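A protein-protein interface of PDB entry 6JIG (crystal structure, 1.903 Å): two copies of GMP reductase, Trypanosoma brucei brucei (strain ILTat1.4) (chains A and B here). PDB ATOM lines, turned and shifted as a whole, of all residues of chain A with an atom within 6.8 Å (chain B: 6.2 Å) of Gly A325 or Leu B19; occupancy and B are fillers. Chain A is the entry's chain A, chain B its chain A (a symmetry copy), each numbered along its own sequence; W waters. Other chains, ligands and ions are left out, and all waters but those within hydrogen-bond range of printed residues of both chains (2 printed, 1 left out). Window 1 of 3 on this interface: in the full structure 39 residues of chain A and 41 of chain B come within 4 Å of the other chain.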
ATOM      1  N   ILE A   9     -19.816  24.826  20.187  1.00  0.00           N
ATOM      2  CA  ILE A   9     -18.455  25.256  20.497  1.00  0.00           C
ATOM      3  C   ILE A   9     -18.256  26.678  19.971  1.00  0.00           C
ATOM      4  O   ILE A   9     -18.467  26.933  18.774  1.00  0.00           O
ATOM      5  CB  ILE A   9     -17.439  24.263  19.910  1.00  0.00           C
ATOM      6  CG1 ILE A   9     -17.649  22.877  20.554  1.00  0.00           C
ATOM      7  CG2 ILE A   9     -16.013  24.756  20.116  1.00  0.00           C
ATOM      8  CD1 ILE A   9     -16.820  21.762  19.949  1.00  0.00           C
ATOM      9  N   VAL A 312      -1.935  31.948  25.938  1.00  0.00           N
ATOM     10  CA  VAL A 312      -1.625  30.526  26.111  1.00  0.00           C
ATOM     11  C   VAL A 312      -1.422  29.943  24.715  1.00  0.00           C
ATOM     12  O   VAL A 312      -2.389  29.728  23.974  1.00  0.00           O
ATOM     13  CB  VAL A 312      -2.725  29.789  26.886  1.00  0.00           C
ATOM     14  CG1 VAL A 312      -2.399  28.282  27.010  1.00  0.00           C
ATOM     15  CG2 VAL A 312      -2.887  30.397  28.273  1.00  0.00           C
ATOM     16  N   ILE A 319       4.690  25.785  21.207  1.00  0.00           N
ATOM     17  CA  ILE A 319       3.972  24.645  20.635  1.00  0.00           C
ATOM     18  C   ILE A 319       3.163  23.920  21.706  1.00  0.00           C
ATOM     19  O   ILE A 319       2.841  22.732  21.561  1.00  0.00           O
ATOM     20  CB  ILE A 319       4.928  23.663  19.929  1.00  0.00           C
ATOM     21  CG1 ILE A 319       6.025  23.194  20.882  1.00  0.00           C
ATOM     22  CG2 ILE A 319       5.534  24.296  18.673  1.00  0.00           C
ATOM     23  CD1 ILE A 319       6.884  22.089  20.311  1.00  0.00           C
ATOM     24  N   THR A 320       2.837  24.635  22.787  1.00  0.00           N
ATOM     25  CA  THR A 320       1.843  24.168  23.746  1.00  0.00           C
ATOM     26  C   THR A 320       0.583  23.647  23.063  1.00  0.00           C
ATOM     27  O   THR A 320      -0.001  22.646  23.488  1.00  0.00           O
ATOM     28  CB  THR A 320       1.493  25.315  24.696  1.00  0.00           C
ATOM     29  OG1 THR A 320       2.638  25.628  25.502  1.00  0.00           O
ATOM     30  CG2 THR A 320       0.314  24.973  25.584  1.00  0.00           C
ATOM     31  N   ARG A 321       0.115  24.350  22.035  1.00  0.00           N
ATOM     32  CA  ARG A 321      -1.090  23.918  21.350  1.00  0.00           C
ATOM     33  C   ARG A 321      -0.867  22.597  20.617  1.00  0.00           C
ATOM     34  O   ARG A 321      -1.819  21.835  20.428  1.00  0.00           O
ATOM     35  CB  ARG A 321      -1.567  25.029  20.398  1.00  0.00           C
ATOM     36  CG  ARG A 321      -1.904  26.331  21.147  1.00  0.00           C
ATOM     37  CD  ARG A 321      -2.343  27.478  20.234  1.00  0.00           C
ATOM     38  NE  ARG A 321      -2.594  28.718  20.974  1.00  0.00           N
ATOM     39  CZ  ARG A 321      -3.089  29.824  20.426  1.00  0.00           C
ATOM     40  NH1 ARG A 321      -3.406  29.849  19.125  1.00  0.00           N
ATOM     41  NH2 ARG A 321      -3.272  30.901  21.175  1.00  0.00           N
ATOM     42  N   LEU A 322       0.377  22.291  20.229  1.00  0.00           N
ATOM     43  CA  LEU A 322       0.654  21.022  19.559  1.00  0.00           C
ATOM     44  C   LEU A 322       0.975  19.899  20.533  1.00  0.00           C
ATOM     45  O   LEU A 322       0.695  18.735  20.224  1.00  0.00           O
ATOM     46  CB  LEU A 322       1.820  21.168  18.577  1.00  0.00           C
ATOM     47  CG  LEU A 322       1.658  22.287  17.539  1.00  0.00           C
ATOM     48  CD1 LEU A 322       2.831  22.304  16.577  1.00  0.00           C
ATOM     49  CD2 LEU A 322       0.347  22.147  16.788  1.00  0.00           C
ATOM     50  N   VAL A 323       1.560  20.212  21.687  1.00  0.00           N
ATOM     51  CA  VAL A 323       1.943  19.177  22.646  1.00  0.00           C
ATOM     52  C   VAL A 323       0.802  18.856  23.603  1.00  0.00           C
ATOM     53  O   VAL A 323       0.469  17.688  23.824  1.00  0.00           O
ATOM     54  CB  VAL A 323       3.216  19.602  23.407  1.00  0.00           C
ATOM     55  CG1 VAL A 323       3.486  18.641  24.544  1.00  0.00           C
ATOM     56  CG2 VAL A 323       4.402  19.648  22.459  1.00  0.00           C
ATOM     57  N   ALA A 324       0.188  19.882  24.190  1.00  0.00           N
ATOM     58  CA  ALA A 324      -0.933  19.688  25.108  1.00  0.00           C
ATOM     59  C   ALA A 324      -2.295  19.826  24.440  1.00  0.00           C
ATOM     60  O   ALA A 324      -3.280  19.290  24.959  1.00  0.00           O
ATOM     61  CB  ALA A 324      -0.848  20.697  26.263  1.00  0.00           C
ATOM     62  N   GLY A 325      -2.379  20.544  23.324  1.00  0.00           N
ATOM     63  CA  GLY A 325      -3.648  20.733  22.647  1.00  0.00           C
ATOM     64  C   GLY A 325      -4.475  21.886  23.170  1.00  0.00           C
ATOM     65  O   GLY A 325      -5.637  22.029  22.760  1.00  0.00           O
ATOM     66  N   ALA A 326      -3.907  22.717  24.049  1.00  0.00           N
ATOM     67  CA  ALA A 326      -4.622  23.746  24.787  1.00  0.00           C
ATOM     68  C   ALA A 326      -4.218  25.138  24.318  1.00  0.00           C
ATOM     69  O   ALA A 326      -3.086  25.360  23.880  1.00  0.00           O
ATOM     70  CB  ALA A 326      -4.343  23.644  26.295  1.00  0.00           C
ATOM     71  N   GLY A 327      -5.137  26.078  24.459  1.00  0.00           N
ATOM     72  CA  GLY A 327      -4.889  27.446  24.046  1.00  0.00           C
ATOM     73  C   GLY A 327      -6.193  28.151  23.723  1.00  0.00           C
ATOM     74  O   GLY A 327      -7.277  27.567  23.753  1.00  0.00           O
ATOM     75  N   VAL A 328      -6.066  29.446  23.444  1.00  0.00           N
ATOM     76  CA  VAL A 328      -7.191  30.287  23.035  1.00  0.00           C
ATOM     77  C   VAL A 328      -6.657  31.249  21.983  1.00  0.00           C
ATOM     78  O   VAL A 328      -5.608  31.872  22.203  1.00  0.00           O
ATOM     79  CB  VAL A 328      -7.801  31.067  24.215  1.00  0.00           C
ATOM     80  CG1 VAL A 328      -8.966  31.953  23.720  1.00  0.00           C
ATOM     81  CG2 VAL A 328      -8.283  30.141  25.305  1.00  0.00           C
ATOM     82  N   PRO A 329      -7.325  31.390  20.835  1.00  0.00           N
ATOM     83  CA  PRO A 329      -6.892  32.375  19.838  1.00  0.00           C
ATOM     84  C   PRO A 329      -6.758  33.744  20.487  1.00  0.00           C
ATOM     85  O   PRO A 329      -7.608  34.159  21.275  1.00  0.00           O
ATOM     86  CB  PRO A 329      -8.019  32.332  18.793  1.00  0.00           C
ATOM     87  CG  PRO A 329      -8.476  30.842  18.875  1.00  0.00           C
ATOM     88  CD  PRO A 329      -8.472  30.590  20.371  1.00  0.00           C
ATOM     89  N   TYR B  15      -9.694  17.608  14.663  1.00  0.00           N
ATOM     90  CA  TYR B  15      -8.817  18.037  15.756  1.00  0.00           C
ATOM     91  C   TYR B  15      -8.234  19.415  15.486  1.00  0.00           C
ATOM     92  O   TYR B  15      -8.195  20.264  16.384  1.00  0.00           O
ATOM     93  CB  TYR B  15      -7.688  17.036  15.976  1.00  0.00           C
ATOM     94  CG  TYR B  15      -8.196  15.663  16.354  1.00  0.00           C
ATOM     95  CD1 TYR B  15      -9.030  15.498  17.452  1.00  0.00           C
ATOM     96  CD2 TYR B  15      -7.865  14.543  15.602  1.00  0.00           C
ATOM     97  CE1 TYR B  15      -9.504  14.240  17.807  1.00  0.00           C
ATOM     98  CE2 TYR B  15      -8.342  13.264  15.957  1.00  0.00           C
ATOM     99  CZ  TYR B  15      -9.159  13.137  17.057  1.00  0.00           C
ATOM    100  OH  TYR B  15      -9.639  11.908  17.437  1.00  0.00           O
ATOM    101  N   ASP B  17      -9.488  21.836  14.142  1.00  0.00           N
ATOM    102  CA  ASP B  17     -10.464  22.915  14.242  1.00  0.00           C
ATOM    103  C   ASP B  17     -10.602  23.488  15.650  1.00  0.00           C
ATOM    104  O   ASP B  17     -11.258  24.520  15.813  1.00  0.00           O
ATOM    105  CB  ASP B  17     -11.853  22.446  13.786  1.00  0.00           C
ATOM    106  CG  ASP B  17     -11.959  22.279  12.262  1.00  0.00           C
ATOM    107  OD1 ASP B  17     -11.622  23.234  11.527  1.00  0.00           O
ATOM    108  OD2 ASP B  17     -12.381  21.191  11.802  1.00  0.00           O
ATOM    109  N   VAL B  18     -10.053  22.845  16.682  1.00  0.00           N
ATOM    110  CA  VAL B  18     -10.340  23.274  18.047  1.00  0.00           C
ATOM    111  C   VAL B  18      -9.068  23.317  18.889  1.00  0.00           C
ATOM    112  O   VAL B  18      -8.040  22.723  18.555  1.00  0.00           O
ATOM    113  CB  VAL B  18     -11.403  22.369  18.731  1.00  0.00           C
ATOM    114  CG1 VAL B  18     -12.725  22.416  17.955  1.00  0.00           C
ATOM    115  CG2 VAL B  18     -10.911  20.926  18.830  1.00  0.00           C
ATOM    116  N   LEU B  19      -9.151  24.070  19.981  1.00  0.00           N
ATOM    117  CA  LEU B  19      -8.181  24.001  21.071  1.00  0.00           C
ATOM    118  C   LEU B  19      -8.918  23.707  22.360  1.00  0.00           C
ATOM    119  O   LEU B  19     -10.101  24.020  22.485  1.00  0.00           O
ATOM    120  CB  LEU B  19      -7.416  25.317  21.231  1.00  0.00           C
ATOM    121  CG  LEU B  19      -6.605  25.751  20.025  1.00  0.00           C
ATOM    122  CD1 LEU B  19      -6.180  27.199  20.257  1.00  0.00           C
ATOM    123  CD2 LEU B  19      -5.391  24.846  19.858  1.00  0.00           C
ATOM    124  N   ILE B  20      -8.209  23.100  23.316  1.00  0.00           N
ATOM    125  CA  ILE B  20      -8.726  22.911  24.669  1.00  0.00           C
ATOM    126  C   ILE B  20      -8.608  24.227  25.433  1.00  0.00           C
ATOM    127  O   ILE B  20      -7.531  24.817  25.508  1.00  0.00           O
ATOM    128  CB  ILE B  20      -7.967  21.793  25.389  1.00  0.00           C
ATOM    129  CG1 ILE B  20      -8.216  20.457  24.679  1.00  0.00           C
ATOM    130  CG2 ILE B  20      -8.361  21.731  26.880  1.00  0.00           C
ATOM    131  CD1 ILE B  20      -7.190  19.374  25.087  1.00  0.00           C
ATOM    132  N   ILE B  21      -9.720  24.702  25.969  1.00  0.00           N
ATOM    133  CA  ILE B  21      -9.711  25.966  26.708  1.00  0.00           C
ATOM    134  C   ILE B  21      -9.078  25.719  28.071  1.00  0.00           C
ATOM    135  O   ILE B  21      -9.523  24.807  28.790  1.00  0.00           O
ATOM    136  CB  ILE B  21     -11.134  26.504  26.876  1.00  0.00           C
ATOM    137  CG1 ILE B  21     -11.781  26.829  25.526  1.00  0.00           C
ATOM    138  CG2 ILE B  21     -11.115  27.770  27.743  1.00  0.00           C
ATOM    139  CD1 ILE B  21     -13.290  27.037  25.642  1.00  0.00           C
ATOM    140  N   SER B 357       0.677  14.649  20.311  1.00  0.00           N
ATOM    141  CA  SER B 357       0.097  14.394  21.621  1.00  0.00           C
ATOM    142  C   SER B 357      -1.047  15.357  21.905  1.00  0.00           C
ATOM    143  O   SER B 357      -2.011  14.986  22.587  1.00  0.00           O
ATOM    144  CB  SER B 357       1.166  14.486  22.720  1.00  0.00           C
ATOM    145  OG  SER B 357       1.837  15.741  22.721  1.00  0.00           O
ATOM    146  N   GLY B 358      -0.978  16.581  21.359  1.00  0.00           N
ATOM    147  CA  GLY B 358      -2.087  17.514  21.521  1.00  0.00           C
ATOM    148  C   GLY B 358      -3.397  16.974  20.976  1.00  0.00           C
ATOM    149  O   GLY B 358      -4.461  17.180  21.565  1.00  0.00           O
ATOM    150  N   ASP B 359      -3.342  16.275  19.844  1.00  0.00           N
ATOM    151  CA  ASP B 359      -4.552  15.657  19.298  1.00  0.00           C
ATOM    152  C   ASP B 359      -5.096  14.574  20.224  1.00  0.00           C
ATOM    153  O   ASP B 359      -6.319  14.383  20.329  1.00  0.00           O
ATOM    154  CB  ASP B 359      -4.259  15.053  17.927  1.00  0.00           C
ATOM    155  CG  ASP B 359      -3.829  16.081  16.908  1.00  0.00           C
ATOM    156  OD1 ASP B 359      -4.125  17.276  17.110  1.00  0.00           O
ATOM    157  OD2 ASP B 359      -3.197  15.681  15.901  1.00  0.00           O
ATOM    158  N   SER B 361      -4.899  14.617  23.530  1.00  0.00           N
ATOM    159  CA  SER B 361      -5.649  15.343  24.554  1.00  0.00           C
ATOM    160  C   SER B 361      -7.032  15.737  24.050  1.00  0.00           C
ATOM    161  O   SER B 361      -8.019  15.647  24.788  1.00  0.00           O
ATOM    162  CB  SER B 361      -4.893  16.596  25.011  1.00  0.00           C
ATOM    163  OG  SER B 361      -3.557  16.319  25.422  1.00  0.00           O
ATOM    164  N   LYS B 362      -7.123  16.204  22.803  1.00  0.00           N
ATOM    165  CA  LYS B 362      -8.428  16.595  22.283  1.00  0.00           C
ATOM    166  C   LYS B 362      -9.356  15.393  22.162  1.00  0.00           C
ATOM    167  O   LYS B 362     -10.548  15.489  22.470  1.00  0.00           O
ATOM    168  CB  LYS B 362      -8.270  17.282  20.919  1.00  0.00           C
ATOM    169  CG  LYS B 362      -7.425  18.559  20.982  1.00  0.00           C
ATOM    170  CD  LYS B 362      -7.193  19.167  19.566  1.00  0.00           C
ATOM    171  CE  LYS B 362      -6.087  20.216  19.602  1.00  0.00           C
ATOM    172  NZ  LYS B 362      -5.917  20.866  18.244  1.00  0.00           N
ATOM    173  N   GLY B 450       2.625  14.446  26.908  1.00  0.00           N
ATOM    174  CA  GLY B 450       1.834  15.507  26.304  1.00  0.00           C
ATOM    175  C   GLY B 450       0.384  15.454  26.742  1.00  0.00           C
ATOM    176  O   GLY B 450      -0.201  16.472  27.114  1.00  0.00           O
ATOM    177  N   GLY B 454      -2.033  18.270  28.636  1.00  0.00           N
ATOM    178  CA  GLY B 454      -3.383  18.692  28.295  1.00  0.00           C
ATOM    179  C   GLY B 454      -4.369  18.474  29.428  1.00  0.00           C
ATOM    180  O   GLY B 454      -5.252  19.297  29.663  1.00  0.00           O
ATOM    181  N   ARG B 471     -13.424  21.731  27.770  1.00  0.00           N
ATOM    182  CA  ARG B 471     -14.214  22.631  26.946  1.00  0.00           C
ATOM    183  C   ARG B 471     -13.355  23.043  25.766  1.00  0.00           C
ATOM    184  O   ARG B 471     -12.155  23.271  25.921  1.00  0.00           O
ATOM    185  CB  ARG B 471     -14.656  23.883  27.720  1.00  0.00           C
ATOM    186  CG  ARG B 471     -15.453  23.575  28.981  1.00  0.00           C
ATOM    187  CD  ARG B 471     -16.820  22.974  28.647  1.00  0.00           C
ATOM    188  NE  ARG B 471     -17.605  22.764  29.860  1.00  0.00           N
ATOM    189  CZ  ARG B 471     -17.679  21.605  30.509  1.00  0.00           C
ATOM    190  NH1 ARG B 471     -17.035  20.538  30.049  1.00  0.00           N
ATOM    191  NH2 ARG B 471     -18.404  21.507  31.616  1.00  0.00           N
ATOM    192  N   PHE B 472     -13.964  23.134  24.593  1.00  0.00           N
ATOM    193  CA  PHE B 472     -13.244  23.471  23.378  1.00  0.00           C
ATOM    194  C   PHE B 472     -13.594  24.880  22.907  1.00  0.00           C
ATOM    195  O   PHE B 472     -14.681  25.395  23.181  1.00  0.00           O
ATOM    196  CB  PHE B 472     -13.577  22.497  22.243  1.00  0.00           C
ATOM    197  CG  PHE B 472     -13.100  21.083  22.490  1.00  0.00           C
ATOM    198  CD1 PHE B 472     -11.753  20.773  22.422  1.00  0.00           C
ATOM    199  CD2 PHE B 472     -14.005  20.077  22.769  1.00  0.00           C
ATOM    200  CE1 PHE B 472     -11.311  19.471  22.625  1.00  0.00           C
ATOM    201  CE2 PHE B 472     -13.576  18.771  22.976  1.00  0.00           C
ATOM    202  CZ  PHE B 472     -12.228  18.471  22.905  1.00  0.00           C
ATOM    203  N   VAL B 473     -12.663  25.470  22.167  1.00  0.00           N
ATOM    204  CA  VAL B 473     -12.910  26.677  21.382  1.00  0.00           C
ATOM    205  C   VAL B 473     -12.476  26.403  19.950  1.00  0.00           C
ATOM    206  O   VAL B 473     -11.433  25.782  19.711  1.00  0.00           O
ATOM    207  CB  VAL B 473     -12.180  27.906  21.985  1.00  0.00           C
ATOM    208  CG1 VAL B 473     -10.674  27.645  22.159  1.00  0.00           C
ATOM    209  CG2 VAL B 473     -12.418  29.154  21.138  1.00  0.00           C
ATOM    210  N   ARG B 474     -13.299  26.832  18.997  1.00  0.00           N
ATOM    211  CA  ARG B 474     -13.030  26.617  17.584  1.00  0.00           C
ATOM    212  C   ARG B 474     -12.077  27.688  17.065  1.00  0.00           C
ATOM    213  O   ARG B 474     -12.123  28.836  17.508  1.00  0.00           O
ATOM    214  CB  ARG B 474     -14.360  26.640  16.830  1.00  0.00           C
ATOM    215  CG  ARG B 474     -14.271  26.478  15.352  1.00  0.00           C
ATOM    216  CD  ARG B 474     -15.626  26.052  14.839  1.00  0.00           C
ATOM    217  NE  ARG B 474     -15.690  26.158  13.395  1.00  0.00           N
ATOM    218  CZ  ARG B 474     -16.830  26.110  12.728  1.00  0.00           C
ATOM    219  NH1 ARG B 474     -17.970  25.970  13.406  1.00  0.00           N
ATOM    220  NH2 ARG B 474     -16.827  26.207  11.409  1.00  0.00           N
ATOM    221  N   MET B 475     -11.161  27.305  16.177  1.00  0.00           N
ATOM    222  CA  MET B 475     -10.261  28.279  15.572  1.00  0.00           C
ATOM    223  C   MET B 475     -10.417  28.265  14.057  1.00  0.00           C
ATOM    224  O   MET B 475     -10.806  27.251  13.465  1.00  0.00           O
ATOM    225  CB  MET B 475      -8.778  28.045  15.977  1.00  0.00           C
ATOM    226  CG  MET B 475      -8.280  26.611  15.935  1.00  0.00           C
ATOM    227  SD  MET B 475      -6.512  26.524  16.363  1.00  0.00           S
ATOM    228  CE  MET B 475      -6.265  24.747  16.402  1.00  0.00           C
ATOM    229  N   GLY B 479      -6.219  31.119  13.147  1.00  0.00           N
ATOM    230  CA  GLY B 479      -5.905  30.632  14.480  1.00  0.00           C
ATOM    231  C   GLY B 479      -5.008  29.408  14.458  1.00  0.00           C
ATOM    232  O   GLY B 479      -4.105  29.271  15.289  1.00  0.00           O
ATOM    233  N   SER B 483      -0.994  28.613  15.980  1.00  0.00           N
ATOM    234  CA  SER B 483      -0.898  27.576  16.996  1.00  0.00           C
ATOM    235  C   SER B 483       0.415  26.800  16.891  1.00  0.00           C
ATOM    236  O   SER B 483       1.011  26.446  17.919  1.00  0.00           O
ATOM    237  CB  SER B 483      -2.128  26.673  16.884  1.00  0.00           C
ATOM    238  OG  SER B 483      -3.278  27.455  17.230  1.00  0.00           O
HETATM  239  O   HOH W   1     -18.861  25.197  16.162  1.00  0.00           O
HETATM  240  O   HOH W   2      -3.548  22.452  18.074  1.00  0.00           O
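Thr A320 touches none of the printed residues of chain B. Gly A325 touches four residues of chain B. Of the printed residues of chain B, Ala A326 touches Ile B20 (3.2 Å). Printed residues of chain A within 4 Å of Gly B479: Arg A321. The nearest residue of chain B that does not touch Gly A325 is Ser B361 (4.9 Å). The nearest residue of chain A that does not touch Leu B19 is Pro A329 (4.1 Å). The nearest printed residue of chain A that does not touch Val B473 is Pro A329 (4.1 Å).
Water W2 bridges the side-chain amino group of Lys B362 and the backbone carbonyl oxygen of Arg A321. Water W1 lies within hydrogen-bond range of NH1 of Arg B474 (3.0 Å) and O of Ile A9 (3.2 Å).
Hydrophobic or aromatic side chains of chain B that line the printed part of chain A: Leu B19, Ile B20, Phe B472 and Val B473. Along chain A the printed residues that touch a printed residue of chain B span positions 9 to 328. Among the printed residues, no Asp or Glu carboxylate lies within 4 Å of a Lys or Arg side-chain nitrogen of the other chain.
CG2 of Ile A9 touches CA of Val B473 (3.9 Å). Ile A9 touches Arg B474 (CG2 to N, 3.6 Å). Leu B19 touches Arg A321 (CD1 to CD, 3.8 Å). Arg A321 touches Gly B479 (NH1 to O, 3.9 Å). Ala A324 touches Ile B20. Ala A324 touches Gly B454. Gly A325 touches Leu B19 (O to CA, 3.6 Å). O of Gly A325 touches CE of Lys B362 (3.7 Å). Val B473 touches Gly A327. Val A328 touches Leu B19.
The backbone carbonyl oxygen (O) of Ile B20 is in hydrogen-bond range of the backbone NH (N) of Gly A327 (2.9 Å). O of Leu A322 sits at hydrogen-bond distance from N of Gly B358 (3.0 Å). O of Val A323 lies within hydrogen-bond range of OG of Ser B357. The backbone carbonyl oxygen (O) of Val A323 lies within hydrogen-bond range of the backbone NH (N) of Gly B358 (3.1 Å). The backbone carbonyl oxygen (O) of Ala A324 lies within hydrogen-bond range of the side-chain hydroxyl (OG) of Ser B361 (3.0 Å). The backbone carbonyl oxygen (O) of Gly A325 sits at hydrogen-bond distance from the backbone NH (N) of Ile B20. The side-chain hydroxyl (OG) of Ser B483 lies within hydrogen-bond range of the guanidinium group (NH1) of Arg A321 (3.1 Å).
O of Thr A320 is in hydrogen-bond range of N of Gly A325 (3.2 Å). The guanidinium group (NH2) of Arg A321 lies within hydrogen-bond range of the backbone carbonyl oxygen (O) of Val A312. The backbone carbonyl oxygen of Tyr B15 sits at hydrogen-bond distance from the side-chain amino group of Lys B362. The backbone carbonyl oxygen (O) of Gly B479 sits at hydrogen-bond distance from the side-chain hydroxyl (OG) of Ser B483, at 2.8 Å. The side-chain amino group (NZ) of Lys B362 sits at hydrogen-bond distance from the backbone carbonyl oxygen (O) of Val B18 (2.8 Å). The backbone NH (N) of Leu B19 sits at hydrogen-bond distance from the backbone carbonyl oxygen (O) of Val B473 (2.9 Å).
No position is printed for both chains.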
